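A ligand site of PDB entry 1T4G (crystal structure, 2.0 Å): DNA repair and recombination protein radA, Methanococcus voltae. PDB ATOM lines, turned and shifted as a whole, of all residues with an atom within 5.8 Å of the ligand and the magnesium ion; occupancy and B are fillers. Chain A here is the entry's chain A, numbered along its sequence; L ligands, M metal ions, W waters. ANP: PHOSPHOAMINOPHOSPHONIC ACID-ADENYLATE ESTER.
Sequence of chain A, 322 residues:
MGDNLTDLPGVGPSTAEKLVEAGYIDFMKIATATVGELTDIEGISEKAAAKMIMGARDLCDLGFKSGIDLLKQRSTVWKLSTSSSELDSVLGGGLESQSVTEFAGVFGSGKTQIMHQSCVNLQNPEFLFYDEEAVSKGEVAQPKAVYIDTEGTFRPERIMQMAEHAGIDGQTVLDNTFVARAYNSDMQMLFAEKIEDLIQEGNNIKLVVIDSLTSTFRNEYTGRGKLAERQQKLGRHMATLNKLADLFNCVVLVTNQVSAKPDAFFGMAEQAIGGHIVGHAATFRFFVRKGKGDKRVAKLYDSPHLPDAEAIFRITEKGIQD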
ATOM      1  N   GLY A 105     -24.729 -37.908   8.704  1.00  0.00           N
ATOM      2  CA  GLY A 105     -24.221 -38.195   7.386  1.00  0.00           C
ATOM      3  C   GLY A 105     -22.740 -37.953   7.234  1.00  0.00           C
ATOM      4  O   GLY A 105     -22.126 -37.223   8.020  1.00  0.00           O
ATOM      5  N   VAL A 106     -22.182 -38.565   6.186  1.00  0.00           N
ATOM      6  CA  VAL A 106     -20.764 -38.438   5.902  1.00  0.00           C
ATOM      7  C   VAL A 106     -20.414 -36.994   5.537  1.00  0.00           C
ATOM      8  O   VAL A 106     -21.303 -36.173   5.269  1.00  0.00           O
ATOM      9  CB  VAL A 106     -20.353 -39.370   4.729  1.00  0.00           C
ATOM     10  CG1 VAL A 106     -20.713 -40.822   5.081  1.00  0.00           C
ATOM     11  CG2 VAL A 106     -21.054 -38.957   3.438  1.00  0.00           C
ATOM     12  N   PHE A 107     -19.121 -36.684   5.553  1.00  0.00           N
ATOM     13  CA  PHE A 107     -18.618 -35.368   5.195  1.00  0.00           C
ATOM     14  C   PHE A 107     -19.233 -34.921   3.883  1.00  0.00           C
ATOM     15  O   PHE A 107     -19.242 -35.684   2.914  1.00  0.00           O
ATOM     16  CB  PHE A 107     -17.099 -35.425   5.013  1.00  0.00           C
ATOM     17  CG  PHE A 107     -16.330 -35.671   6.275  1.00  0.00           C
ATOM     18  CD1 PHE A 107     -16.075 -34.634   7.163  1.00  0.00           C
ATOM     19  CD2 PHE A 107     -15.819 -36.930   6.551  1.00  0.00           C
ATOM     20  CE1 PHE A 107     -15.328 -34.851   8.321  1.00  0.00           C
ATOM     21  CE2 PHE A 107     -15.067 -37.171   7.703  1.00  0.00           C
ATOM     22  CZ  PHE A 107     -14.818 -36.122   8.587  1.00  0.00           C
ATOM     23  N   GLY A 108     -19.735 -33.696   3.844  1.00  0.00           N
ATOM     24  CA  GLY A 108     -20.302 -33.161   2.612  1.00  0.00           C
ATOM     25  C   GLY A 108     -21.619 -33.728   2.102  1.00  0.00           C
ATOM     26  O   GLY A 108     -22.013 -33.422   0.977  1.00  0.00           O
ATOM     27  N   SER A 109     -22.302 -34.535   2.898  1.00  0.00           N
ATOM     28  CA  SER A 109     -23.576 -35.106   2.454  1.00  0.00           C
ATOM     29  C   SER A 109     -24.715 -34.081   2.383  1.00  0.00           C
ATOM     30  O   SER A 109     -25.750 -34.355   1.769  1.00  0.00           O
ATOM     31  CB  SER A 109     -23.975 -36.257   3.371  1.00  0.00           C
ATOM     32  OG  SER A 109     -24.025 -35.843   4.717  1.00  0.00           O
ATOM     33  N   GLY A 110     -24.548 -32.919   3.001  1.00  0.00           N
ATOM     34  CA  GLY A 110     -25.588 -31.897   2.928  1.00  0.00           C
ATOM     35  C   GLY A 110     -26.279 -31.492   4.221  1.00  0.00           C
ATOM     36  O   GLY A 110     -27.248 -30.727   4.197  1.00  0.00           O
ATOM     37  N   LYS A 111     -25.789 -31.990   5.353  1.00  0.00           N
ATOM     38  CA  LYS A 111     -26.371 -31.676   6.657  1.00  0.00           C
ATOM     39  C   LYS A 111     -26.555 -30.159   6.870  1.00  0.00           C
ATOM     40  O   LYS A 111     -27.643 -29.702   7.210  1.00  0.00           O
ATOM     41  CB  LYS A 111     -25.472 -32.233   7.770  1.00  0.00           C
ATOM     42  CG  LYS A 111     -25.210 -33.735   7.673  1.00  0.00           C
ATOM     43  CD  LYS A 111     -24.366 -34.240   8.838  1.00  0.00           C
ATOM     44  CE  LYS A 111     -22.933 -33.716   8.789  1.00  0.00           C
ATOM     45  NZ  LYS A 111     -22.264 -34.176   7.538  1.00  0.00           N
ATOM     46  N   THR A 112     -25.503 -29.395   6.650  1.00  0.00           N
ATOM     47  CA  THR A 112     -25.545 -27.949   6.829  1.00  0.00           C
ATOM     48  C   THR A 112     -26.502 -27.286   5.834  1.00  0.00           C
ATOM     49  O   THR A 112     -27.230 -26.351   6.167  1.00  0.00           O
ATOM     50  CB  THR A 112     -24.113 -27.360   6.720  1.00  0.00           C
ATOM     51  OG1 THR A 112     -23.345 -27.860   7.820  1.00  0.00           O
ATOM     52  CG2 THR A 112     -24.122 -25.841   6.775  1.00  0.00           C
ATOM     53  N   GLN A 113     -26.494 -27.780   4.599  1.00  0.00           N
ATOM     54  CA  GLN A 113     -27.411 -27.248   3.577  1.00  0.00           C
ATOM     55  C   GLN A 113     -28.847 -27.400   4.057  1.00  0.00           C
ATOM     56  O   GLN A 113     -29.668 -26.486   3.915  1.00  0.00           O
ATOM     57  CB  GLN A 113     -27.246 -27.988   2.247  1.00  0.00           C
ATOM     58  CG  GLN A 113     -25.916 -27.747   1.547  1.00  0.00           C
ATOM     59  CD  GLN A 113     -25.659 -26.269   1.298  1.00  0.00           C
ATOM     60  OE1 GLN A 113     -26.348 -25.616   0.520  1.00  0.00           O
ATOM     61  NE2 GLN A 113     -24.654 -25.730   1.980  1.00  0.00           N
ATOM     62  N   ILE A 114     -29.173 -28.556   4.619  1.00  0.00           N
ATOM     63  CA  ILE A 114     -30.530 -28.767   5.098  1.00  0.00           C
ATOM     64  C   ILE A 114     -30.862 -27.789   6.216  1.00  0.00           C
ATOM     65  O   ILE A 114     -31.979 -27.269   6.279  1.00  0.00           O
ATOM     66  CB  ILE A 114     -30.723 -30.224   5.574  1.00  0.00           C
ATOM     67  CG1 ILE A 114     -30.551 -31.167   4.373  1.00  0.00           C
ATOM     68  CG2 ILE A 114     -32.113 -30.392   6.164  1.00  0.00           C
ATOM     69  CD1 ILE A 114     -30.307 -32.619   4.748  1.00  0.00           C
ATOM     70  N   GLU A 151     -19.585 -25.223  13.984  1.00  0.00           N
ATOM     71  CA  GLU A 151     -18.566 -25.520  12.987  1.00  0.00           C
ATOM     72  C   GLU A 151     -17.982 -24.264  12.324  1.00  0.00           C
ATOM     73  O   GLU A 151     -16.849 -24.282  11.845  1.00  0.00           O
ATOM     74  CB  GLU A 151     -19.154 -26.408  11.890  1.00  0.00           C
ATOM     75  CG  GLU A 151     -19.984 -27.588  12.367  1.00  0.00           C
ATOM     76  CD  GLU A 151     -19.146 -28.687  12.996  1.00  0.00           C
ATOM     77  OE1 GLU A 151     -19.178 -29.832  12.490  1.00  0.00           O
ATOM     78  OE2 GLU A 151     -18.457 -28.396  13.998  1.00  0.00           O
ATOM     79  N   THR A 153     -19.755 -22.757   9.873  1.00  0.00           N
ATOM     80  CA  THR A 153     -20.193 -22.850   8.494  1.00  0.00           C
ATOM     81  C   THR A 153     -21.532 -22.190   8.172  1.00  0.00           C
ATOM     82  O   THR A 153     -22.167 -22.510   7.147  1.00  0.00           O
ATOM     83  CB  THR A 153     -20.205 -24.321   8.019  1.00  0.00           C
ATOM     84  OG1 THR A 153     -20.846 -25.142   9.007  1.00  0.00           O
ATOM     85  CG2 THR A 153     -18.778 -24.801   7.803  1.00  0.00           C
ATOM     86  N   ARG A 158     -25.658 -18.023   1.328  1.00  0.00           N
ATOM     87  CA  ARG A 158     -26.443 -19.190   0.957  1.00  0.00           C
ATOM     88  C   ARG A 158     -27.900 -18.985   1.341  1.00  0.00           C
ATOM     89  O   ARG A 158     -28.809 -19.430   0.636  1.00  0.00           O
ATOM     90  CB  ARG A 158     -25.889 -20.432   1.654  1.00  0.00           C
ATOM     91  CG  ARG A 158     -26.460 -21.738   1.162  1.00  0.00           C
ATOM     92  CD  ARG A 158     -26.245 -21.923  -0.338  1.00  0.00           C
ATOM     93  NE  ARG A 158     -26.664 -23.261  -0.749  1.00  0.00           N
ATOM     94  CZ  ARG A 158     -27.247 -23.557  -1.908  1.00  0.00           C
ATOM     95  NH1 ARG A 158     -27.595 -24.803  -2.172  1.00  0.00           N
ATOM     96  NH2 ARG A 158     -27.492 -22.593  -2.787  1.00  0.00           N
ATOM     97  N   GLN A 161     -29.362 -16.676  -1.334  1.00  0.00           N
ATOM     98  CA  GLN A 161     -29.552 -17.417  -2.569  1.00  0.00           C
ATOM     99  C   GLN A 161     -30.758 -18.361  -2.512  1.00  0.00           C
ATOM    100  O   GLN A 161     -31.599 -18.365  -3.423  1.00  0.00           O
ATOM    101  CB  GLN A 161     -28.276 -18.206  -2.892  1.00  0.00           C
ATOM    102  CG  GLN A 161     -28.312 -18.981  -4.193  1.00  0.00           C
ATOM    103  CD  GLN A 161     -26.967 -19.624  -4.501  1.00  0.00           C
ATOM    104  OE1 GLN A 161     -26.343 -20.254  -3.639  1.00  0.00           O
ATOM    105  NE2 GLN A 161     -26.514 -19.489  -5.744  1.00  0.00           N
ATOM    106  N   ASP A 211     -25.887 -27.237  14.601  1.00  0.00           N
ATOM    107  CA  ASP A 211     -24.982 -27.780  13.586  1.00  0.00           C
ATOM    108  C   ASP A 211     -23.567 -27.407  13.998  1.00  0.00           C
ATOM    109  O   ASP A 211     -23.160 -26.278  13.799  1.00  0.00           O
ATOM    110  CB  ASP A 211     -25.343 -27.169  12.217  1.00  0.00           C
ATOM    111  CG  ASP A 211     -24.490 -27.683  11.089  1.00  0.00           C
ATOM    112  OD1 ASP A 211     -24.218 -28.902  11.059  1.00  0.00           O
ATOM    113  OD2 ASP A 211     -24.113 -26.875  10.213  1.00  0.00           O
ATOM    114  N   GLN A 257     -22.069 -35.749  12.179  1.00  0.00           N
ATOM    115  CA  GLN A 257     -21.252 -36.314  11.140  1.00  0.00           C
ATOM    116  C   GLN A 257     -20.842 -37.729  11.519  1.00  0.00           C
ATOM    117  O   GLN A 257     -20.338 -37.978  12.608  1.00  0.00           O
ATOM    118  CB  GLN A 257     -20.018 -35.444  10.953  1.00  0.00           C
ATOM    119  CG  GLN A 257     -19.108 -35.904   9.878  1.00  0.00           C
ATOM    120  CD  GLN A 257     -17.793 -35.200   9.974  1.00  0.00           C
ATOM    121  OE1 GLN A 257     -17.663 -34.049   9.564  1.00  0.00           O
ATOM    122  NE2 GLN A 257     -16.818 -35.870  10.577  1.00  0.00           N
ATOM    123  N   LYS A 290     -24.121 -39.182  -0.282  1.00  0.00           N
ATOM    124  CA  LYS A 290     -24.155 -38.569  -1.595  1.00  0.00           C
ATOM    125  C   LYS A 290     -24.559 -39.554  -2.680  1.00  0.00           C
ATOM    126  O   LYS A 290     -24.273 -40.746  -2.593  1.00  0.00           O
ATOM    127  CB  LYS A 290     -22.786 -38.013  -1.982  1.00  0.00           C
ATOM    128  CG  LYS A 290     -22.263 -36.880  -1.129  1.00  0.00           C
ATOM    129  CD  LYS A 290     -21.042 -36.272  -1.817  1.00  0.00           C
ATOM    130  CE  LYS A 290     -20.392 -35.194  -0.973  1.00  0.00           C
ATOM    131  NZ  LYS A 290     -19.228 -34.587  -1.688  1.00  0.00           N
ATOM    132  N   ARG A 296     -28.535 -36.803  -3.591  1.00  0.00           N
ATOM    133  CA  ARG A 296     -28.333 -37.093  -2.178  1.00  0.00           C
ATOM    134  C   ARG A 296     -29.415 -38.111  -1.804  1.00  0.00           C
ATOM    135  O   ARG A 296     -30.534 -38.058  -2.321  1.00  0.00           O
ATOM    136  CB  ARG A 296     -28.497 -35.825  -1.356  1.00  0.00           C
ATOM    137  CG  ARG A 296     -27.490 -34.727  -1.688  1.00  0.00           C
ATOM    138  CD  ARG A 296     -26.102 -35.065  -1.175  1.00  0.00           C
ATOM    139  NE  ARG A 296     -25.180 -33.959  -1.376  1.00  0.00           N
ATOM    140  CZ  ARG A 296     -24.568 -33.699  -2.533  1.00  0.00           C
ATOM    141  NH1 ARG A 296     -24.784 -34.474  -3.595  1.00  0.00           N
ATOM    142  NH2 ARG A 296     -23.776 -32.642  -2.631  1.00  0.00           N
ATOM    143  N   ILE A 315     -29.223 -31.231  -4.234  1.00  0.00           N
ATOM    144  CA  ILE A 315     -28.839 -29.944  -3.670  1.00  0.00           C
ATOM    145  C   ILE A 315     -28.241 -29.161  -4.835  1.00  0.00           C
ATOM    146  O   ILE A 315     -27.244 -29.576  -5.427  1.00  0.00           O
ATOM    147  CB  ILE A 315     -27.801 -30.115  -2.536  1.00  0.00           C
ATOM    148  CG1 ILE A 315     -28.414 -30.904  -1.365  1.00  0.00           C
ATOM    149  CG2 ILE A 315     -27.340 -28.750  -2.052  1.00  0.00           C
ATOM    150  CD1 ILE A 315     -27.515 -31.026  -0.130  1.00  0.00           C
ATOM    151  N   THR A 316     -28.881 -28.047  -5.176  1.00  0.00           N
ATOM    152  CA  THR A 316     -28.438 -27.209  -6.287  1.00  0.00           C
ATOM    153  C   THR A 316     -28.297 -25.794  -5.757  1.00  0.00           C
ATOM    154  O   THR A 316     -28.326 -25.580  -4.551  1.00  0.00           O
ATOM    155  CB  THR A 316     -29.487 -27.204  -7.397  1.00  0.00           C
ATOM    156  OG1 THR A 316     -30.669 -26.565  -6.915  1.00  0.00           O
ATOM    157  CG2 THR A 316     -29.828 -28.643  -7.817  1.00  0.00           C
ATOM    158  N   GLU A 317     -28.154 -24.819  -6.658  1.00  0.00           N
ATOM    159  CA  GLU A 317     -28.037 -23.438  -6.225  1.00  0.00           C
ATOM    160  C   GLU A 317     -29.346 -22.967  -5.606  1.00  0.00           C
ATOM    161  O   GLU A 317     -29.373 -21.959  -4.904  1.00  0.00           O
ATOM    162  CB  GLU A 317     -27.667 -22.512  -7.389  1.00  0.00           C
ATOM    163  CG  GLU A 317     -27.681 -23.135  -8.763  1.00  0.00           C
ATOM    164  CD  GLU A 317     -29.045 -23.590  -9.215  1.00  0.00           C
ATOM    165  OE1 GLU A 317     -30.011 -22.805  -9.093  1.00  0.00           O
ATOM    166  OE2 GLU A 317     -29.164 -24.737  -9.694  1.00  0.00           O
ATOM    167  N   LYS A 318     -30.423 -23.691  -5.870  1.00  0.00           N
ATOM    168  CA  LYS A 318     -31.718 -23.309  -5.321  1.00  0.00           C
ATOM    169  C   LYS A 318     -31.915 -23.851  -3.905  1.00  0.00           C
ATOM    170  O   LYS A 318     -32.845 -23.459  -3.207  1.00  0.00           O
ATOM    171  CB  LYS A 318     -32.840 -23.818  -6.219  1.00  0.00           C
ATOM    172  CG  LYS A 318     -32.741 -23.316  -7.648  1.00  0.00           C
ATOM    173  CD  LYS A 318     -33.941 -23.734  -8.485  1.00  0.00           C
ATOM    174  CE  LYS A 318     -33.845 -23.167  -9.902  1.00  0.00           C
ATOM    175  NZ  LYS A 318     -35.103 -23.437 -10.677  1.00  0.00           N
HETATM  176  PG  ANP L   1     -19.652 -31.460   6.829  1.00  0.00           P
HETATM  177  O1G ANP L   1     -19.794 -32.776   7.368  1.00  0.00           O
HETATM  178  O2G ANP L   1     -20.160 -30.453   7.807  1.00  0.00           O
HETATM  179  O3G ANP L   1     -18.248 -31.202   6.558  1.00  0.00           O
HETATM  180  PB  ANP L   1     -22.058 -31.223   5.269  1.00  0.00           P
HETATM  181  O1B ANP L   1     -22.581 -30.179   6.198  1.00  0.00           O
HETATM  182  O2B ANP L   1     -22.700 -32.502   5.551  1.00  0.00           O
HETATM  183  N3B ANP L   1     -20.489 -31.361   5.384  1.00  0.00           N
HETATM  184  PA  ANP L   1     -22.778 -29.364   3.294  1.00  0.00           P
HETATM  185  O1A ANP L   1     -24.152 -28.986   3.841  1.00  0.00           O
HETATM  186  O2A ANP L   1     -21.756 -28.376   3.765  1.00  0.00           O
HETATM  187  O3A ANP L   1     -22.386 -30.846   3.758  1.00  0.00           O
HETATM  188  O5' ANP L   1     -22.874 -29.398   1.654  1.00  0.00           O
HETATM  189  C5' ANP L   1     -21.726 -29.072   0.723  1.00  0.00           C
HETATM  190  C4' ANP L   1     -22.184 -29.222  -0.520  1.00  0.00           C
HETATM  191  O4' ANP L   1     -23.373 -28.359  -0.714  1.00  0.00           O
HETATM  192  C3' ANP L   1     -21.187 -28.642  -1.565  1.00  0.00           C
HETATM  193  O3' ANP L   1     -19.972 -29.292  -1.658  1.00  0.00           O
HETATM  194  C2' ANP L   1     -22.079 -28.205  -2.758  1.00  0.00           C
HETATM  195  O2' ANP L   1     -22.219 -29.408  -3.698  1.00  0.00           O
HETATM  196  C1' ANP L   1     -23.455 -27.963  -2.113  1.00  0.00           C
HETATM  197  N9  ANP L   1     -23.630 -26.609  -2.163  1.00  0.00           N
HETATM  198  C8  ANP L   1     -23.343 -25.668  -1.140  1.00  0.00           C
HETATM  199  N7  ANP L   1     -23.608 -24.474  -1.556  1.00  0.00           N
HETATM  200  C5  ANP L   1     -24.064 -24.550  -2.827  1.00  0.00           C
HETATM  201  C6  ANP L   1     -24.480 -23.611  -3.754  1.00  0.00           C
HETATM  202  N6  ANP L   1     -24.479 -22.286  -3.434  1.00  0.00           N
HETATM  203  N1  ANP L   1     -24.906 -24.037  -5.020  1.00  0.00           N
HETATM  204  C2  ANP L   1     -24.906 -25.416  -5.366  1.00  0.00           C
HETATM  205  N3  ANP L   1     -24.497 -26.363  -4.492  1.00  0.00           N
HETATM  206  C4  ANP L   1     -24.076 -25.882  -3.223  1.00  0.00           C
HETATM  207 MG    MG M   1     -21.718 -29.206   7.724  1.00  0.00          MG
HETATM  208  O   HOH W   1     -23.891 -31.737   0.185  1.00  0.00           O
HETATM  209  O   HOH W   2     -16.834 -32.053   4.532  1.00  0.00           O
HETATM  210  O   HOH W   3     -20.751 -28.122   9.123  1.00  0.00           O
HETATM  211  O   HOH W   4     -20.682 -31.523  10.934  1.00  0.00           O
HETATM  212  O   HOH W   5     -22.644 -30.127   9.393  1.00  0.00           O
HETATM  213  O   HOH W   6     -22.764 -25.870   3.721  1.00  0.00           O
HETATM  214  O   HOH W   7     -20.282 -31.232  -3.095  1.00  0.00           O
HETATM  215  O   HOH W   8     -18.152 -28.427   6.520  1.00  0.00           O
HETATM  216  O   HOH W   9     -20.092 -32.162  -0.684  1.00  0.00           O
HETATM  217  O   HOH W  10     -18.367 -29.063   9.912  1.00  0.00           O
HETATM  218  O   HOH W  11     -20.858 -28.049   6.367  1.00  0.00           O
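N of Thr 112 lies within hydrogen-bond range of O1A of the ligand, 3.1 Å away.
An oxygen (O2B) of the ligand is in hydrogen-bond range of the backbone NH (N) of Lys 111 (3.1 Å).
An oxygen (O2B) of the ligand is in salt-bridge range of the side-chain amino group of Lys 111 (2.6 Å).
N of Gln 113 lies within hydrogen-bond range of O1A of the ligand, at 2.7 Å.
The side-chain amide oxygen of Gln 161 is in hydrogen-bond range of a nitrogen (N6) of the ligand (2.8 Å).
N of Gly 110 lies within hydrogen-bond range of O3A of the ligand, at 3.1 Å.
N7 of the ligand sits at hydrogen-bond distance from NE of Arg 158, at 3.4 Å.
OE1 of Gln 257 lies close to O1G of the ligand, 3.3 Å away.
An oxygen (O2B) of the ligand sits at hydrogen-bond distance from the backbone NH (N) of Ser 109, at 3.4 Å.
The side-chain carboxylate (OD2) of Asp 211 lies close to the side-chain hydroxyl (OG1) of Thr 112 (2.7 Å).
O of Val 106 sits at hydrogen-bond distance from NZ of Lys 111 (3.2 Å).
O of Gly 105 lies within hydrogen-bond range of NZ of Lys 111 (3.1 Å).
The side-chain amide oxygen (OE1) of Gln 161 sits at hydrogen-bond distance from the guanidinium group (NH2) of Arg 158 (2.7 Å).
The guanidinium group (NH2) of Arg 158 sits at hydrogen-bond distance from the backbone carbonyl oxygen (O) of Glu 317 (2.9 Å).
NH1 of Arg 158 lies within hydrogen-bond range of O of Thr 316 (2.6 Å).
O of Val 106 lies within hydrogen-bond range of OG of Ser 109 (2.8 Å).
N of Lys 318 lies close to OG1 of Thr 316, 3.1 Å away.
The backbone NH of Gly 108 lies close to a nitrogen (N3B) of the ligand (2.9 Å).
Merely in contact with the ligand: Glu 317, Thr 316, Phe 107, Arg 296, Val 106 and Ile 315.
15 residues have an atom within 4 Å of the ligand: Val 106, Phe 107, Gly 108, Ser 109, Gly 110, Lys 111, Thr 112, Gln 113, Arg 158, Gln 161, Gln 257, Arg 296, Ile 315, Thr 316 and Glu 317.
The nearest printed residue that does not touch the ligand is Glu 151 (4.8 Å).
Within 4 Å of the magnesium ion: Thr 112.
The nearest printed residue that does not touch the magnesium ion is Asp 211 (4.2 Å).
The magnesium ion is bound by water W11, O2G of the ligand, O1B of the ligand, water W3, OG1 of Thr 112 and water W5.
The magnesium ion has six donor atoms within binding distance.
Water W2 lies within hydrogen-bond range of O3G of the ligand (2.6 Å) and N of Gly 108 (3.4 Å).
Water W6 bridges NE2 of Gln 113 (2.6 Å) and O2A of the ligand (2.7 Å).
Water W1 lies within hydrogen-bond range of the backbone carbonyl oxygen (O) of Gly 108 (2.6 Å), an oxygen (O5') of the ligand (2.9 Å), the guanidinium group (NH2) of Arg 296 (3.0 Å) and the backbone NH (N) of Gly 110 (3.1 Å).
Water W9 lies within hydrogen-bond range of NZ of Lys 290, O of Gly 108 and O3' of the ligand.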
